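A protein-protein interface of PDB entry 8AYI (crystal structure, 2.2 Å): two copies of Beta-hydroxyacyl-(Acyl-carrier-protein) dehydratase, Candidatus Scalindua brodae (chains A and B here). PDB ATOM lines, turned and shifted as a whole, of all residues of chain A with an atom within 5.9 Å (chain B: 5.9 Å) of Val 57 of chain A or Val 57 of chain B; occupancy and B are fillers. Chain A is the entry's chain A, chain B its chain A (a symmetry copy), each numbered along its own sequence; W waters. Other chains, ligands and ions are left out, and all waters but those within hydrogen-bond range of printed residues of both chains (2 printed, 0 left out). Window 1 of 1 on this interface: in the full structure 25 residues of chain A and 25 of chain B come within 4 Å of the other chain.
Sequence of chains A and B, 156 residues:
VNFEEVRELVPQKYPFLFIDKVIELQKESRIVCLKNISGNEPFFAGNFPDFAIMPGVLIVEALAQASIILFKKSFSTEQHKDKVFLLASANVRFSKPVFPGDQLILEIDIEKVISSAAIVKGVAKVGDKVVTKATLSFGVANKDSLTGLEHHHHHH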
ATOM      1  N   PHE A  16      27.424 -13.092  10.834  1.00  0.00           N
ATOM      2  CA  PHE A  16      26.124 -13.011  10.178  1.00  0.00           C
ATOM      3  C   PHE A  16      25.417 -14.362  10.164  1.00  0.00           C
ATOM      4  O   PHE A  16      24.610 -14.638   9.272  1.00  0.00           O
ATOM      5  CB  PHE A  16      26.263 -12.466   8.758  1.00  0.00           C
ATOM      6  CG  PHE A  16      25.082 -11.661   8.304  1.00  0.00           C
ATOM      7  CD1 PHE A  16      24.834 -10.414   8.851  1.00  0.00           C
ATOM      8  CD2 PHE A  16      24.224 -12.146   7.332  1.00  0.00           C
ATOM      9  CE1 PHE A  16      23.750  -9.665   8.441  1.00  0.00           C
ATOM     10  CE2 PHE A  16      23.138 -11.402   6.917  1.00  0.00           C
ATOM     11  CZ  PHE A  16      22.900 -10.159   7.474  1.00  0.00           C
ATOM     12  N   PRO A  55      17.558  -5.805  15.953  1.00  0.00           N
ATOM     13  CA  PRO A  55      17.014  -5.201  14.729  1.00  0.00           C
ATOM     14  C   PRO A  55      16.063  -6.154  14.028  1.00  0.00           C
ATOM     15  O   PRO A  55      16.306  -7.359  13.947  1.00  0.00           O
ATOM     16  CB  PRO A  55      18.261  -4.928  13.879  1.00  0.00           C
ATOM     17  CG  PRO A  55      19.394  -4.923  14.838  1.00  0.00           C
ATOM     18  CD  PRO A  55      19.025  -5.875  15.932  1.00  0.00           C
ATOM     19  N   GLY A  56      14.965  -5.599  13.519  1.00  0.00           N
ATOM     20  CA  GLY A  56      13.970  -6.429  12.863  1.00  0.00           C
ATOM     21  C   GLY A  56      14.492  -7.112  11.617  1.00  0.00           C
ATOM     22  O   GLY A  56      14.091  -8.233  11.306  1.00  0.00           O
ATOM     23  N   VAL A  57      15.392  -6.454  10.886  1.00  0.00           N
ATOM     24  CA  VAL A  57      15.899  -7.030   9.643  1.00  0.00           C
ATOM     25  C   VAL A  57      16.735  -8.272   9.924  1.00  0.00           C
ATOM     26  O   VAL A  57      16.832  -9.163   9.071  1.00  0.00           O
ATOM     27  CB  VAL A  57      16.694  -5.978   8.846  1.00  0.00           C
ATOM     28  CG1 VAL A  57      15.799  -4.805   8.487  1.00  0.00           C
ATOM     29  CG2 VAL A  57      17.901  -5.506   9.642  1.00  0.00           C
ATOM     30  N   LEU A  58      17.341  -8.364  11.112  1.00  0.00           N
ATOM     31  CA  LEU A  58      18.116  -9.554  11.443  1.00  0.00           C
ATOM     32  C   LEU A  58      17.212 -10.734  11.773  1.00  0.00           C
ATOM     33  O   LEU A  58      17.623 -11.887  11.617  1.00  0.00           O
ATOM     34  CB  LEU A  58      19.065  -9.257  12.603  1.00  0.00           C
ATOM     35  CG  LEU A  58      20.111  -8.175  12.317  1.00  0.00           C
ATOM     36  CD1 LEU A  58      21.153  -8.114  13.423  1.00  0.00           C
ATOM     37  CD2 LEU A  58      20.771  -8.411  10.964  1.00  0.00           C
ATOM     38  N   ILE A  59      15.985 -10.468  12.228  1.00  0.00           N
ATOM     39  CA  ILE A  59      15.010 -11.541  12.383  1.00  0.00           C
ATOM     40  C   ILE A  59      14.598 -12.075  11.018  1.00  0.00           C
ATOM     41  O   ILE A  59      14.409 -13.283  10.838  1.00  0.00           O
ATOM     42  CB  ILE A  59      13.796 -11.049  13.191  1.00  0.00           C
ATOM     43  CG1 ILE A  59      14.229 -10.596  14.586  1.00  0.00           C
ATOM     44  CG2 ILE A  59      12.739 -12.139  13.283  1.00  0.00           C
ATOM     45  CD1 ILE A  59      13.093 -10.068  15.434  1.00  0.00           C
ATOM     46  N   VAL A  60      14.453 -11.182  10.035  1.00  0.00           N
ATOM     47  CA  VAL A  60      14.152 -11.610   8.672  1.00  0.00           C
ATOM     48  C   VAL A  60      15.276 -12.481   8.128  1.00  0.00           C
ATOM     49  O   VAL A  60      15.033 -13.480   7.440  1.00  0.00           O
ATOM     50  CB  VAL A  60      13.897 -10.384   7.774  1.00  0.00           C
ATOM     51  CG1 VAL A  60      13.704 -10.809   6.326  1.00  0.00           C
ATOM     52  CG2 VAL A  60      12.690  -9.606   8.273  1.00  0.00           C
ATOM     53  N   GLU A  61      16.525 -12.123   8.435  1.00  0.00           N
ATOM     54  CA  GLU A  61      17.654 -12.935   7.997  1.00  0.00           C
ATOM     55  C   GLU A  61      17.659 -14.291   8.691  1.00  0.00           C
ATOM     56  O   GLU A  61      17.985 -15.310   8.071  1.00  0.00           O
ATOM     57  CB  GLU A  61      18.966 -12.194   8.254  1.00  0.00           C
ATOM     58  CG  GLU A  61      20.212 -12.966   7.851  1.00  0.00           C
ATOM     59  CD  GLU A  61      20.300 -13.211   6.355  1.00  0.00           C
ATOM     60  OE1 GLU A  61      20.988 -14.173   5.949  1.00  0.00           O
ATOM     61  OE2 GLU A  61      19.684 -12.442   5.585  1.00  0.00           O
ATOM     62  N   ALA A  62      17.300 -14.324   9.977  1.00  0.00           N
ATOM     63  CA  ALA A  62      17.210 -15.594  10.687  1.00  0.00           C
ATOM     64  C   ALA A  62      16.142 -16.487  10.074  1.00  0.00           C
ATOM     65  O   ALA A  62      16.336 -17.702   9.944  1.00  0.00           O
ATOM     66  CB  ALA A  62      16.925 -15.345  12.169  1.00  0.00           C
ATOM     67  N   LEU A  87      17.513 -14.561  -1.315  1.00  0.00           N
ATOM     68  CA  LEU A  87      16.279 -13.824  -1.057  1.00  0.00           C
ATOM     69  C   LEU A  87      15.889 -12.970  -2.253  1.00  0.00           C
ATOM     70  O   LEU A  87      16.633 -12.071  -2.658  1.00  0.00           O
ATOM     71  CB  LEU A  87      16.442 -12.942   0.185  1.00  0.00           C
ATOM     72  CG  LEU A  87      15.856 -13.450   1.505  1.00  0.00           C
ATOM     73  CD1 LEU A  87      16.022 -12.416   2.612  1.00  0.00           C
ATOM     74  CD2 LEU A  87      14.393 -13.810   1.325  1.00  0.00           C
ATOM     75  N   PHE A  94       6.664  -6.580  11.720  1.00  0.00           N
ATOM     76  CA  PHE A  94       7.363  -6.720  12.992  1.00  0.00           C
ATOM     77  C   PHE A  94       6.376  -6.409  14.110  1.00  0.00           C
ATOM     78  O   PHE A  94       5.962  -5.257  14.282  1.00  0.00           O
ATOM     79  CB  PHE A  94       8.586  -5.808  13.037  1.00  0.00           C
ATOM     80  CG  PHE A  94       9.482  -5.946  11.838  1.00  0.00           C
ATOM     81  CD1 PHE A  94      10.421  -6.962  11.767  1.00  0.00           C
ATOM     82  CD2 PHE A  94       9.372  -5.065  10.775  1.00  0.00           C
ATOM     83  CE1 PHE A  94      11.238  -7.092  10.657  1.00  0.00           C
ATOM     84  CE2 PHE A  94      10.184  -5.189   9.668  1.00  0.00           C
ATOM     85  CZ  PHE A  94      11.119  -6.204   9.608  1.00  0.00           C
ATOM     86  N   PHE B  16      26.355  -1.287  13.063  1.00  0.00           N
ATOM     87  CA  PHE B  16      25.035  -1.366  12.449  1.00  0.00           C
ATOM     88  C   PHE B  16      24.588  -0.014  11.905  1.00  0.00           C
ATOM     89  O   PHE B  16      23.388   0.264  11.825  1.00  0.00           O
ATOM     90  CB  PHE B  16      24.006  -1.910  13.439  1.00  0.00           C
ATOM     91  CG  PHE B  16      22.916  -2.713  12.793  1.00  0.00           C
ATOM     92  CD1 PHE B  16      23.190  -3.961  12.259  1.00  0.00           C
ATOM     93  CD2 PHE B  16      21.623  -2.226  12.723  1.00  0.00           C
ATOM     94  CE1 PHE B  16      22.195  -4.707  11.662  1.00  0.00           C
ATOM     95  CE2 PHE B  16      20.622  -2.969  12.128  1.00  0.00           C
ATOM     96  CZ  PHE B  16      20.909  -4.212  11.595  1.00  0.00           C
ATOM     97  N   PRO B  55      24.242  -8.564   2.144  1.00  0.00           N
ATOM     98  CA  PRO B  55      22.944  -9.165   2.474  1.00  0.00           C
ATOM     99  C   PRO B  55      21.806  -8.211   2.164  1.00  0.00           C
ATOM    100  O   PRO B  55      21.895  -7.007   2.406  1.00  0.00           O
ATOM    101  CB  PRO B  55      23.049  -9.440   3.980  1.00  0.00           C
ATOM    102  CG  PRO B  55      24.506  -9.447   4.274  1.00  0.00           C
ATOM    103  CD  PRO B  55      25.136  -8.496   3.308  1.00  0.00           C
ATOM    104  N   GLY B  56      20.725  -8.763   1.618  1.00  0.00           N
ATOM    105  CA  GLY B  56      19.595  -7.932   1.245  1.00  0.00           C
ATOM    106  C   GLY B  56      18.942  -7.248   2.428  1.00  0.00           C
ATOM    107  O   GLY B  56      18.450  -6.127   2.307  1.00  0.00           O
ATOM    108  N   VAL B  57      18.924  -7.909   3.587  1.00  0.00           N
ATOM    109  CA  VAL B  57      18.265  -7.332   4.755  1.00  0.00           C
ATOM    110  C   VAL B  57      19.005  -6.091   5.238  1.00  0.00           C
ATOM    111  O   VAL B  57      18.398  -5.199   5.843  1.00  0.00           O
ATOM    112  CB  VAL B  57      18.132  -8.385   5.873  1.00  0.00           C
ATOM    113  CG1 VAL B  57      17.293  -9.556   5.393  1.00  0.00           C
ATOM    114  CG2 VAL B  57      19.504  -8.859   6.326  1.00  0.00           C
ATOM    115  N   LEU B  58      20.314  -6.000   4.976  1.00  0.00           N
ATOM    116  CA  LEU B  58      21.056  -4.812   5.380  1.00  0.00           C
ATOM    117  C   LEU B  58      20.755  -3.632   4.468  1.00  0.00           C
ATOM    118  O   LEU B  58      20.890  -2.478   4.887  1.00  0.00           O
ATOM    119  CB  LEU B  58      22.554  -5.112   5.406  1.00  0.00           C
ATOM    120  CG  LEU B  58      22.976  -6.194   6.402  1.00  0.00           C
ATOM    121  CD1 LEU B  58      24.490  -6.258   6.534  1.00  0.00           C
ATOM    122  CD2 LEU B  58      22.325  -5.958   7.759  1.00  0.00           C
ATOM    123  N   ILE B  59      20.351  -3.896   3.223  1.00  0.00           N
ATOM    124  CA  ILE B  59      19.871  -2.821   2.362  1.00  0.00           C
ATOM    125  C   ILE B  59      18.544  -2.286   2.886  1.00  0.00           C
ATOM    126  O   ILE B  59      18.288  -1.077   2.850  1.00  0.00           O
ATOM    127  CB  ILE B  59      19.750  -3.312   0.908  1.00  0.00           C
ATOM    128  CG1 ILE B  59      21.113  -3.767   0.383  1.00  0.00           C
ATOM    129  CG2 ILE B  59      19.169  -2.220   0.023  1.00  0.00           C
ATOM    130  CD1 ILE B  59      21.073  -4.294  -1.035  1.00  0.00           C
ATOM    131  N   VAL B  60      17.682  -3.178   3.381  1.00  0.00           N
ATOM    132  CA  VAL B  60      16.426  -2.749   3.991  1.00  0.00           C
ATOM    133  C   VAL B  60      16.699  -1.878   5.210  1.00  0.00           C
ATOM    134  O   VAL B  60      16.009  -0.879   5.447  1.00  0.00           O
ATOM    135  CB  VAL B  60      15.562  -3.973   4.346  1.00  0.00           C
ATOM    136  CG1 VAL B  60      14.307  -3.547   5.093  1.00  0.00           C
ATOM    137  CG2 VAL B  60      15.204  -4.750   3.089  1.00  0.00           C
ATOM    138  N   GLU B  61      17.713  -2.239   5.999  1.00  0.00           N
ATOM    139  CA  GLU B  61      18.071  -1.428   7.157  1.00  0.00           C
ATOM    140  C   GLU B  61      18.620  -0.073   6.732  1.00  0.00           C
ATOM    141  O   GLU B  61      18.338   0.947   7.373  1.00  0.00           O
ATOM    142  CB  GLU B  61      19.085  -2.171   8.026  1.00  0.00           C
ATOM    143  CG  GLU B  61      19.543  -1.401   9.255  1.00  0.00           C
ATOM    144  CD  GLU B  61      18.424  -1.155  10.252  1.00  0.00           C
ATOM    145  OE1 GLU B  61      18.534  -0.194  11.043  1.00  0.00           O
ATOM    146  OE2 GLU B  61      17.437  -1.922  10.245  1.00  0.00           O
ATOM    147  N   ALA B  62      19.407  -0.040   5.652  1.00  0.00           N
ATOM    148  CA  ALA B  62      19.910   1.229   5.142  1.00  0.00           C
ATOM    149  C   ALA B  62      18.767   2.125   4.686  1.00  0.00           C
ATOM    150  O   ALA B  62      18.788   3.340   4.919  1.00  0.00           O
ATOM    151  CB  ALA B  62      20.896   0.980   3.999  1.00  0.00           C
ATOM    152  N   LEU B  87      10.681   0.204  12.822  1.00  0.00           N
ATOM    153  CA  LEU B  87      10.116  -0.531  11.694  1.00  0.00           C
ATOM    154  C   LEU B  87       8.935  -1.384  12.129  1.00  0.00           C
ATOM    155  O   LEU B  87       9.078  -2.284  12.964  1.00  0.00           O
ATOM    156  CB  LEU B  87      11.191  -1.413  11.050  1.00  0.00           C
ATOM    157  CG  LEU B  87      11.864  -0.906   9.773  1.00  0.00           C
ATOM    158  CD1 LEU B  87      12.834  -1.942   9.216  1.00  0.00           C
ATOM    159  CD2 LEU B  87      10.816  -0.544   8.737  1.00  0.00           C
ATOM    160  N   PHE B  94      14.167  -7.769  -3.778  1.00  0.00           N
ATOM    161  CA  PHE B  94      15.599  -7.632  -4.017  1.00  0.00           C
ATOM    162  C   PHE B  94      15.864  -7.943  -5.486  1.00  0.00           C
ATOM    163  O   PHE B  94      15.740  -9.093  -5.918  1.00  0.00           O
ATOM    164  CB  PHE B  94      16.391  -8.546  -3.088  1.00  0.00           C
ATOM    165  CG  PHE B  94      16.007  -8.408  -1.641  1.00  0.00           C
ATOM    166  CD1 PHE B  94      16.534  -7.393  -0.859  1.00  0.00           C
ATOM    167  CD2 PHE B  94      15.103  -9.288  -1.069  1.00  0.00           C
ATOM    168  CE1 PHE B  94      16.171  -7.264   0.470  1.00  0.00           C
ATOM    169  CE2 PHE B  94      14.738  -9.164   0.256  1.00  0.00           C
ATOM    170  CZ  PHE B  94      15.273  -8.151   1.027  1.00  0.00           C
HETATM  171  O   HOH W   1      15.962  -3.714  11.671  1.00  0.00           O
HETATM  172  O   HOH W   2      19.891 -10.649   3.545  1.00  0.00           O
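Among the printed residues, pairs that only touch across the chains: Pro 55 of chain A with Phe 16 of chain B (3.5 Å), Phe 16 of chain A with Pro 55 of chain B (3.5 Å), Val 57 of chain A with Val 57 of chain B (3.5 Å), Leu 87 of chain A with Phe 94 of chain B (3.6 Å), Phe 94 of chain A with Leu 87 of chain B (3.6 Å), Glu 61 of chain A with Val 57 of chain B (3.7 Å), Val 57 of chain A with Glu 61 of chain B (3.7 Å), Val 57 of chain A with Phe 16 of chain B (3.8 Å), Phe 16 of chain A with Val 57 of chain B (3.8 Å), Val 60 of chain A with Val 57 of chain B (3.9 Å), Val 57 of chain A with Val 60 of chain B (3.9 Å), Phe 16 of chain A with Leu 58 of chain B (3.97 Å) and Leu 58 of chain A with Phe 16 of chain B (3.97 Å).
Of the 11 printed residues of chain B, 8 touch a printed residue of chain A. Hydrophobic or aromatic side chains of chain B that line the printed part of chain A: Phe 16, Pro 55, Val 57, Leu 58, Val 60 and Phe 94. Of the 11 printed residues of chain A, 8 touch a printed residue of chain B. Among the printed residues, 13 pairs touch across the chains. Among the printed residues, no Asp or Glu carboxylate lies within 4 Å of a Lys or Arg side-chain nitrogen of the other chain.
Water W2 lies within hydrogen-bond range of the side-chain carboxylate (OE2) of Glu 61 of chain A (2.7 Å), the backbone NH (N) of Gly 56 of chain B (2.8 Å) and the backbone NH (N) of Val 57 of chain B (2.9 Å). Water W1 lies within hydrogen-bond range of OE2 of Glu 61 of chain B (2.7 Å), N of Gly 56 of chain A (2.8 Å) and N of Val 57 of chain A (2.9 Å).
Phe 16 of chain A touches Val 57 of chain B, and with the chains exchanged Val 57 of chain A touches Phe 16 of chain B. Phe 16 of chain A touches Leu 58 of chain B, and with the chains exchanged Leu 58 of chain A touches Phe 16 of chain B. Val 57 of chain B touches its own counterpart, Val 57 of chain A. Val 57 of chain A touches Val 60 of chain B, and with the chains exchanged Val 60 of chain A touches Val 57 of chain B. 11 positions are printed for both chains. Of the 13 pairs that touch across the chains among the printed residues, 13 have their exchanged pair printed and touching as well.
Of the printed residues of chain B, Val 57 of chain A touches Phe 16 (3.8 Å), Val 57 (3.5 Å), Val 60 (3.9 Å) and Glu 61 (3.7 Å). Of the printed residues of chain B, Glu 61 of chain A touches Val 57 (3.7 Å). Val 57 of chain B touches just these residues of chain A: Phe 16 (3.8 Å), Val 57 (3.5 Å), Val 60 (3.9 Å) and Glu 61 (3.7 Å). Printed residues of chain A within 4 Å of Glu 61 of chain B: Val 57. Of the printed residues of chain A, Leu 87 of chain B touches Phe 94.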
